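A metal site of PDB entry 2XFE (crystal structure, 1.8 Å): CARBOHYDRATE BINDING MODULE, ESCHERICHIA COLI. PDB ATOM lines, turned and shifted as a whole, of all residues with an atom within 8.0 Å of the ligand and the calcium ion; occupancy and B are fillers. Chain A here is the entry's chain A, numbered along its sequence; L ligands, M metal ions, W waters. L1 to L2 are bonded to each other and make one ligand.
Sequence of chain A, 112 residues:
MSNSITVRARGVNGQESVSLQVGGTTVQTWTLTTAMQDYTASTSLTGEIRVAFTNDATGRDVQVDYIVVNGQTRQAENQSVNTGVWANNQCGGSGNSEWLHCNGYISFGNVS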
ATOM      1  N   VAL A  12      -8.961  -9.628  31.615  1.00  0.00           N
ATOM      2  CA  VAL A  12      -9.985  -9.262  30.625  1.00  0.00           C
ATOM      3  C   VAL A  12     -11.361  -9.143  31.294  1.00  0.00           C
ATOM      4  O   VAL A  12     -12.162  -8.245  30.971  1.00  0.00           O
ATOM      5  CB  VAL A  12      -9.941 -10.322  29.483  1.00  0.00           C
ATOM      6  CG1 VAL A  12     -11.230 -10.298  28.692  1.00  0.00           C
ATOM      7  CG2 VAL A  12      -8.673 -10.122  28.633  1.00  0.00           C
ATOM      8  N   GLU A  16      -9.919 -13.044  37.074  1.00  0.00           N
ATOM      9  CA  GLU A  16      -8.686 -13.793  36.888  1.00  0.00           C
ATOM     10  C   GLU A  16      -7.848 -13.776  38.150  1.00  0.00           C
ATOM     11  O   GLU A  16      -7.763 -12.782  38.819  1.00  0.00           O
ATOM     12  CB  GLU A  16      -7.870 -13.216  35.695  1.00  0.00           C
ATOM     13  CG  GLU A  16      -8.498 -13.385  34.331  1.00  0.00           C
ATOM     14  CD  GLU A  16      -9.467 -12.265  33.892  1.00  0.00           C
ATOM     15  OE1 GLU A  16      -9.764 -11.327  34.687  1.00  0.00           O
ATOM     16  OE2 GLU A  16      -9.865 -12.322  32.737  1.00  0.00           O
ATOM     17  N   PHE A  53      -1.113 -17.720  36.146  1.00  0.00           N
ATOM     18  CA  PHE A  53      -2.544 -17.626  35.961  1.00  0.00           C
ATOM     19  C   PHE A  53      -3.073 -19.052  36.200  1.00  0.00           C
ATOM     20  O   PHE A  53      -2.578 -20.037  35.577  1.00  0.00           O
ATOM     21  CB  PHE A  53      -2.792 -17.173  34.555  1.00  0.00           C
ATOM     22  CG  PHE A  53      -4.189 -17.156  34.118  1.00  0.00           C
ATOM     23  CD1 PHE A  53      -5.258 -16.885  34.964  1.00  0.00           C
ATOM     24  CD2 PHE A  53      -4.448 -17.350  32.767  1.00  0.00           C
ATOM     25  CE1 PHE A  53      -6.564 -16.806  34.459  1.00  0.00           C
ATOM     26  CE2 PHE A  53      -5.731 -17.257  32.236  1.00  0.00           C
ATOM     27  CZ  PHE A  53      -6.782 -16.953  33.043  1.00  0.00           C
ATOM     28  N   ASN A  55      -6.749 -19.931  36.981  1.00  0.00           N
ATOM     29  CA  ASN A  55      -8.208 -20.152  36.918  1.00  0.00           C
ATOM     30  C   ASN A  55      -8.786 -19.835  35.528  1.00  0.00           C
ATOM     31  O   ASN A  55      -9.904 -19.319  35.365  1.00  0.00           O
ATOM     32  CB  ASN A  55      -8.884 -19.395  38.057  1.00  0.00           C
ATOM     33  CG  ASN A  55      -8.918 -17.910  37.867  1.00  0.00           C
ATOM     34  OD1 ASN A  55      -8.035 -17.319  37.230  1.00  0.00           O
ATOM     35  ND2 ASN A  55      -9.876 -17.270  38.497  1.00  0.00           N
ATOM     36  N   ASP A  56      -8.047 -20.195  34.468  1.00  0.00           N
ATOM     37  CA  ASP A  56      -8.565 -20.024  33.136  1.00  0.00           C
ATOM     38  C   ASP A  56      -9.974 -20.611  33.024  1.00  0.00           C
ATOM     39  O   ASP A  56     -10.285 -21.660  33.600  1.00  0.00           O
ATOM     40  CB  ASP A  56      -7.633 -20.629  32.117  1.00  0.00           C
ATOM     41  CG  ASP A  56      -7.949 -20.242  30.713  1.00  0.00           C
ATOM     42  OD1 ASP A  56      -8.403 -19.106  30.551  1.00  0.00           O
ATOM     43  OD2 ASP A  56      -7.715 -21.078  29.807  1.00  0.00           O
ATOM     44  N   ALA A  57     -10.826 -19.900  32.278  1.00  0.00           N
ATOM     45  CA  ALA A  57     -12.230 -20.324  31.986  1.00  0.00           C
ATOM     46  C   ALA A  57     -12.654 -19.537  30.743  1.00  0.00           C
ATOM     47  O   ALA A  57     -11.981 -18.606  30.313  1.00  0.00           O
ATOM     48  CB  ALA A  57     -13.135 -19.982  33.142  1.00  0.00           C
ATOM     49  N   THR A  58     -13.787 -19.914  30.165  1.00  0.00           N
ATOM     50  CA  THR A  58     -14.297 -19.222  29.030  1.00  0.00           C
ATOM     51  C   THR A  58     -14.402 -17.777  29.410  1.00  0.00           C
ATOM     52  O   THR A  58     -15.097 -17.452  30.325  1.00  0.00           O
ATOM     53  CB  THR A  58     -15.654 -19.862  28.568  1.00  0.00           C
ATOM     54  OG1 THR A  58     -15.403 -21.252  28.239  1.00  0.00           O
ATOM     55  CG2 THR A  58     -16.170 -19.121  27.334  1.00  0.00           C
ATOM     56  N   GLY A  59     -13.647 -16.884  28.726  1.00  0.00           N
ATOM     57  CA  GLY A  59     -13.705 -15.454  28.937  1.00  0.00           C
ATOM     58  C   GLY A  59     -12.621 -14.770  29.824  1.00  0.00           C
ATOM     59  O   GLY A  59     -12.565 -13.571  29.916  1.00  0.00           O
ATOM     60  N   ARG A  60     -11.708 -15.573  30.400  1.00  0.00           N
ATOM     61  CA  ARG A  60     -10.667 -15.068  31.304  1.00  0.00           C
ATOM     62  C   ARG A  60      -9.269 -15.140  30.591  1.00  0.00           C
ATOM     63  O   ARG A  60      -8.948 -16.156  30.047  1.00  0.00           O
ATOM     64  CB  ARG A  60     -10.585 -15.938  32.564  1.00  0.00           C
ATOM     65  CG  ARG A  60     -11.866 -15.897  33.443  1.00  0.00           C
ATOM     66  CD  ARG A  60     -11.685 -16.728  34.680  1.00  0.00           C
ATOM     67  NE  ARG A  60     -12.867 -16.775  35.502  1.00  0.00           N
ATOM     68  CZ  ARG A  60     -13.146 -17.701  36.374  1.00  0.00           C
ATOM     69  NH1 ARG A  60     -12.377 -18.763  36.514  1.00  0.00           N
ATOM     70  NH2 ARG A  60     -14.278 -17.571  37.068  1.00  0.00           N
ATOM     71  N   ASP A  61      -8.481 -14.082  30.680  1.00  0.00           N
ATOM     72  CA  ASP A  61      -7.102 -13.991  30.169  1.00  0.00           C
ATOM     73  C   ASP A  61      -6.356 -12.993  31.028  1.00  0.00           C
ATOM     74  O   ASP A  61      -6.965 -12.021  31.477  1.00  0.00           O
ATOM     75  CB  ASP A  61      -6.989 -13.429  28.748  1.00  0.00           C
ATOM     76  CG  ASP A  61      -7.545 -14.359  27.663  1.00  0.00           C
ATOM     77  OD1 ASP A  61      -7.984 -13.828  26.635  1.00  0.00           O
ATOM     78  OD2 ASP A  61      -7.433 -15.590  27.793  1.00  0.00           O
ATOM     79  N   VAL A  62      -5.057 -13.219  31.238  1.00  0.00           N
ATOM     80  CA  VAL A  62      -4.230 -12.343  32.080  1.00  0.00           C
ATOM     81  C   VAL A  62      -3.212 -11.656  31.205  1.00  0.00           C
ATOM     82  O   VAL A  62      -2.709 -12.268  30.222  1.00  0.00           O
ATOM     83  CB  VAL A  62      -3.578 -13.149  33.224  1.00  0.00           C
ATOM     84  CG1 VAL A  62      -2.455 -12.334  33.864  1.00  0.00           C
ATOM     85  CG2 VAL A  62      -4.642 -13.559  34.262  1.00  0.00           C
ATOM     86  N   GLY A  84       1.661 -19.945  29.311  1.00  0.00           N
ATOM     87  CA  GLY A  84       0.244 -19.682  29.157  1.00  0.00           C
ATOM     88  C   GLY A  84      -0.161 -18.881  27.943  1.00  0.00           C
ATOM     89  O   GLY A  84      -1.309 -18.889  27.581  1.00  0.00           O
ATOM     90  N   VAL A  85       0.786 -18.250  27.260  1.00  0.00           N
ATOM     91  CA  VAL A  85       0.439 -17.482  26.087  1.00  0.00           C
ATOM     92  C   VAL A  85      -0.112 -18.375  24.942  1.00  0.00           C
ATOM     93  O   VAL A  85       0.453 -19.426  24.632  1.00  0.00           O
ATOM     94  CB  VAL A  85       1.673 -16.700  25.602  1.00  0.00           C
ATOM     95  CG1 VAL A  85       2.834 -17.635  25.243  1.00  0.00           C
ATOM     96  CG2 VAL A  85       1.315 -15.756  24.418  1.00  0.00           C
ATOM     97  N   TRP A  86      -1.176 -17.951  24.303  1.00  0.00           N
ATOM     98  CA  TRP A  86      -1.632 -18.524  23.040  1.00  0.00           C
ATOM     99  C   TRP A  86      -0.774 -17.994  21.884  1.00  0.00           C
ATOM    100  O   TRP A  86      -0.773 -16.806  21.586  1.00  0.00           O
ATOM    101  CB  TRP A  86      -3.093 -18.175  22.791  1.00  0.00           C
ATOM    102  CG  TRP A  86      -3.651 -18.848  21.611  1.00  0.00           C
ATOM    103  CD1 TRP A  86      -3.851 -18.317  20.351  1.00  0.00           C
ATOM    104  CD2 TRP A  86      -4.071 -20.193  21.540  1.00  0.00           C
ATOM    105  NE1 TRP A  86      -4.409 -19.281  19.525  1.00  0.00           N
ATOM    106  CE2 TRP A  86      -4.528 -20.440  20.235  1.00  0.00           C
ATOM    107  CE3 TRP A  86      -4.160 -21.204  22.470  1.00  0.00           C
ATOM    108  CZ2 TRP A  86      -5.041 -21.638  19.854  1.00  0.00           C
ATOM    109  CZ3 TRP A  86      -4.669 -22.440  22.061  1.00  0.00           C
ATOM    110  CH2 TRP A  86      -5.052 -22.637  20.759  1.00  0.00           C
ATOM    111  N   ALA A  87      -0.030 -18.860  21.256  1.00  0.00           N
ATOM    112  CA  ALA A  87       0.866 -18.457  20.187  1.00  0.00           C
ATOM    113  C   ALA A  87       1.115 -19.738  19.360  1.00  0.00           C
ATOM    114  O   ALA A  87       1.040 -20.879  19.861  1.00  0.00           O
ATOM    115  CB  ALA A  87       2.143 -17.952  20.761  1.00  0.00           C
ATOM    116  N   ASN A  89      -0.721 -21.224  17.503  1.00  0.00           N
ATOM    117  CA  ASN A  89      -1.965 -22.024  17.544  1.00  0.00           C
ATOM    118  C   ASN A  89      -1.983 -23.041  18.703  1.00  0.00           C
ATOM    119  O   ASN A  89      -2.476 -24.207  18.544  1.00  0.00           O
ATOM    120  CB  ASN A  89      -2.219 -22.724  16.210  1.00  0.00           C
ATOM    121  CG  ASN A  89      -3.656 -23.199  16.059  1.00  0.00           C
ATOM    122  OD1 ASN A  89      -4.581 -22.398  16.148  1.00  0.00           O
ATOM    123  ND2 ASN A  89      -3.840 -24.498  15.765  1.00  0.00           N
ATOM    124  N   GLN A  90      -1.423 -22.633  19.842  1.00  0.00           N
ATOM    125  CA  GLN A  90      -1.360 -23.522  21.006  1.00  0.00           C
ATOM    126  C   GLN A  90      -1.099 -22.732  22.292  1.00  0.00           C
ATOM    127  O   GLN A  90      -0.541 -21.665  22.245  1.00  0.00           O
ATOM    128  CB  GLN A  90      -0.232 -24.560  20.853  1.00  0.00           C
ATOM    129  CG  GLN A  90       1.123 -24.020  21.172  1.00  0.00           C
ATOM    130  CD  GLN A  90       2.226 -25.081  21.226  1.00  0.00           C
ATOM    131  OE1 GLN A  90       2.814 -25.369  22.279  1.00  0.00           O
ATOM    132  NE2 GLN A  90       2.536 -25.609  20.087  1.00  0.00           N
ATOM    133  N   CYS A  91      -1.488 -23.323  23.417  1.00  0.00           N
ATOM    134  CA  CYS A  91      -1.209 -22.817  24.764  1.00  0.00           C
ATOM    135  C   CYS A  91       0.269 -22.961  25.039  1.00  0.00           C
ATOM    136  O   CYS A  91       0.852 -23.974  24.680  1.00  0.00           O
ATOM    137  CB  CYS A  91      -1.955 -23.648  25.825  1.00  0.00           C
ATOM    138  SG  CYS A  91      -3.735 -23.390  25.798  1.00  0.00           S
ATOM    139  N   TRP A  99       1.073 -11.856  27.797  1.00  0.00           N
ATOM    140  CA  TRP A  99      -0.225 -12.540  27.919  1.00  0.00           C
ATOM    141  C   TRP A  99      -0.133 -13.940  28.465  1.00  0.00           C
ATOM    142  O   TRP A  99       0.763 -14.721  28.100  1.00  0.00           O
ATOM    143  CB  TRP A  99      -0.959 -12.486  26.583  1.00  0.00           C
ATOM    144  CG  TRP A  99      -1.482 -11.111  26.272  1.00  0.00           C
ATOM    145  CD1 TRP A  99      -0.818 -10.150  25.604  1.00  0.00           C
ATOM    146  CD2 TRP A  99      -2.713 -10.506  26.723  1.00  0.00           C
ATOM    147  NE1 TRP A  99      -1.539  -9.002  25.591  1.00  0.00           N
ATOM    148  CE2 TRP A  99      -2.726  -9.203  26.235  1.00  0.00           C
ATOM    149  CE3 TRP A  99      -3.820 -10.967  27.420  1.00  0.00           C
ATOM    150  CZ2 TRP A  99      -3.774  -8.331  26.493  1.00  0.00           C
ATOM    151  CZ3 TRP A  99      -4.849 -10.098  27.667  1.00  0.00           C
ATOM    152  CH2 TRP A  99      -4.851  -8.831  27.196  1.00  0.00           C
ATOM    153  N   LEU A 100      -1.055 -14.269  29.370  1.00  0.00           N
ATOM    154  CA  LEU A 100      -1.337 -15.629  29.745  1.00  0.00           C
ATOM    155  C   LEU A 100      -2.807 -15.862  29.382  1.00  0.00           C
ATOM    156  O   LEU A 100      -3.704 -15.434  30.106  1.00  0.00           O
ATOM    157  CB  LEU A 100      -1.131 -15.851  31.229  1.00  0.00           C
ATOM    158  CG  LEU A 100       0.325 -15.683  31.672  1.00  0.00           C
ATOM    159  CD1 LEU A 100       0.532 -15.590  33.163  1.00  0.00           C
ATOM    160  CD2 LEU A 100       1.088 -16.907  31.238  1.00  0.00           C
ATOM    161  N   HIS A 101      -3.015 -16.504  28.239  1.00  0.00           N
ATOM    162  CA  HIS A 101      -4.382 -16.863  27.715  1.00  0.00           C
ATOM    163  C   HIS A 101      -4.874 -18.174  28.312  1.00  0.00           C
ATOM    164  O   HIS A 101      -6.049 -18.315  28.634  1.00  0.00           O
ATOM    165  CB  HIS A 101      -4.413 -16.991  26.182  1.00  0.00           C
ATOM    166  CG  HIS A 101      -3.911 -15.783  25.463  1.00  0.00           C
ATOM    167  ND1 HIS A 101      -4.679 -14.661  25.241  1.00  0.00           N
ATOM    168  CD2 HIS A 101      -2.682 -15.517  24.947  1.00  0.00           C
ATOM    169  CE1 HIS A 101      -3.965 -13.754  24.616  1.00  0.00           C
ATOM    170  NE2 HIS A 101      -2.755 -14.267  24.401  1.00  0.00           N
ATOM    171  N   CYS A 102      -3.985 -19.146  28.453  1.00  0.00           N
ATOM    172  CA  CYS A 102      -4.271 -20.397  29.138  1.00  0.00           C
ATOM    173  C   CYS A 102      -3.614 -20.415  30.520  1.00  0.00           C
ATOM    174  O   CYS A 102      -2.731 -19.578  30.822  1.00  0.00           O
ATOM    175  CB  CYS A 102      -3.651 -21.519  28.307  1.00  0.00           C
ATOM    176  SG  CYS A 102      -4.037 -21.435  26.493  1.00  0.00           S
ATOM    177  N   ASN A 103      -4.001 -21.385  31.359  1.00  0.00           N
ATOM    178  CA  ASN A 103      -3.295 -21.552  32.633  1.00  0.00           C
ATOM    179  C   ASN A 103      -1.813 -21.787  32.376  1.00  0.00           C
ATOM    180  O   ASN A 103      -1.456 -22.485  31.437  1.00  0.00           O
ATOM    181  CB  ASN A 103      -3.847 -22.721  33.444  1.00  0.00           C
ATOM    182  CG  ASN A 103      -5.201 -22.417  34.075  1.00  0.00           C
ATOM    183  OD1 ASN A 103      -5.494 -21.274  34.468  1.00  0.00           O
ATOM    184  ND2 ASN A 103      -6.037 -23.468  34.173  1.00  0.00           N
HETATM  185  C1  LIG L   1      -8.775 -16.510  19.962  1.00  0.00           C
HETATM  186  C2  LIG L   1      -8.129 -16.030  21.224  1.00  0.00           C
HETATM  187  C3  LIG L   1      -6.951 -16.924  21.616  1.00  0.00           C
HETATM  188  C4  LIG L   1      -7.379 -18.349  21.805  1.00  0.00           C
HETATM  189  C5  LIG L   1      -8.204 -18.713  20.566  1.00  0.00           C
HETATM  190  C6  LIG L   1      -8.706 -20.136  20.589  1.00  0.00           C
HETATM  191  O1  LIG L   1      -9.813 -15.553  19.635  1.00  0.00           O
HETATM  192  O2  LIG L   1      -7.651 -14.762  20.968  1.00  0.00           O
HETATM  193  O3  LIG L   1      -6.407 -16.457  22.793  1.00  0.00           O
HETATM  194  O4  LIG L   1      -8.178 -18.372  23.012  1.00  0.00           O
HETATM  195  O5  LIG L   1      -9.257 -17.785  20.291  1.00  0.00           O
HETATM  196  O6  LIG L   1      -9.549 -20.263  19.443  1.00  0.00           O
HETATM  197  C1  LG2 L   2      -7.906 -19.442  23.907  1.00  0.00           C
HETATM  198  C2  LG2 L   2      -8.163 -19.129  25.412  1.00  0.00           C
HETATM  199  C3  LG2 L   2      -7.929 -20.229  26.435  1.00  0.00           C
HETATM  200  C4  LG2 L   2      -8.339 -21.615  25.898  1.00  0.00           C
HETATM  201  C5  LG2 L   2      -7.882 -21.780  24.421  1.00  0.00           C
HETATM  202  C6  LG2 L   2      -8.419 -23.121  23.856  1.00  0.00           C
HETATM  203  O1  LG2 L   2      -7.798 -17.849  25.912  1.00  0.00           O
HETATM  204  O2  LG2 L   2      -8.615 -19.865  27.641  1.00  0.00           O
HETATM  205  O3  LG2 L   2      -9.751 -21.836  25.946  1.00  0.00           O
HETATM  206  O4  LG2 L   2      -8.166 -20.752  23.475  1.00  0.00           O
HETATM  207  O5  LG2 L   2      -7.599 -23.500  22.811  1.00  0.00           O
HETATM  208 CA    CA M   1      -8.279 -17.643  28.412  1.00  0.00          CA
HETATM  209  O   HOH W   1      -4.368 -14.962  21.709  1.00  0.00           O
HETATM  210  O   HOH W   2     -11.803 -20.548  24.307  1.00  0.00           O
HETATM  211  O   HOH W   3     -11.129 -18.052  22.904  1.00  0.00           O
HETATM  212  O   HOH W   4     -10.450 -17.258  27.650  1.00  0.00           O
HETATM  213  O   HOH W   5      -8.378 -15.678  24.583  1.00  0.00           O
HETATM  214  O   HOH W   6     -11.245 -21.089  28.439  1.00  0.00           O
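Water W5 bridges an oxygen (O3) of LIG L1 (2.8 Å) and the side-chain carboxylate (OD1) of Asp 61 (2.8 Å). Water W1 bridges O3 of LIG L1 (2.8 Å) and NE2 of His 101 (3.2 Å). Water W6 lies within hydrogen-bond range of O3 of LG2 L2 (3.0 Å), O of Ala 57 (3.2 Å) and N of Thr 58 (3.3 Å).
Trp 86 touches the ligand. Hydrophobic or aromatic side chains that line the ligand: Trp 86 and His 101.
The calcium ion is bound by the side-chain carboxylate (OD2) of Asp 61 (2.3 Å), the backbone carbonyl oxygen (O) of Arg 60 (2.3 Å), water W4 (2.3 Å), the backbone carbonyl oxygen (O) of His 101 (2.3 Å), an oxygen (O2) of LG2 L2 (2.4 Å), an oxygen (O1) of LG2 L2 (2.6 Å) and the side-chain carboxylate (OD1) of Asp 56 (2.6 Å).
O3 of LIG L1 is in hydrogen-bond range of ND1 of His 101, at 3.5 Å.
Of the 23 residues printed, 4 come within 4 Å of the calcium ion. The nearest printed residue that does not touch the calcium ion is Ala 57 (4.3 Å).
OE2 of Glu 16 sits at hydrogen-bond distance from N of Asp 61. The backbone carbonyl oxygen (O) of Asp 61 sits at hydrogen-bond distance from the backbone NH (N) of Val 12 (3.1 Å). The guanidinium group of Arg 60 lies within hydrogen-bond range of the backbone carbonyl oxygen of Asn 55 (2.8 Å). The backbone carbonyl oxygen of Gly 84 lies within hydrogen-bond range of the backbone NH of His 101, 3.0 Å away. N of Asp 56 lies within hydrogen-bond range of OD1 of Asn 103. SG of Cys 91 is disulfide-bonded to SG of Cys 102, 2.1 Å away.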
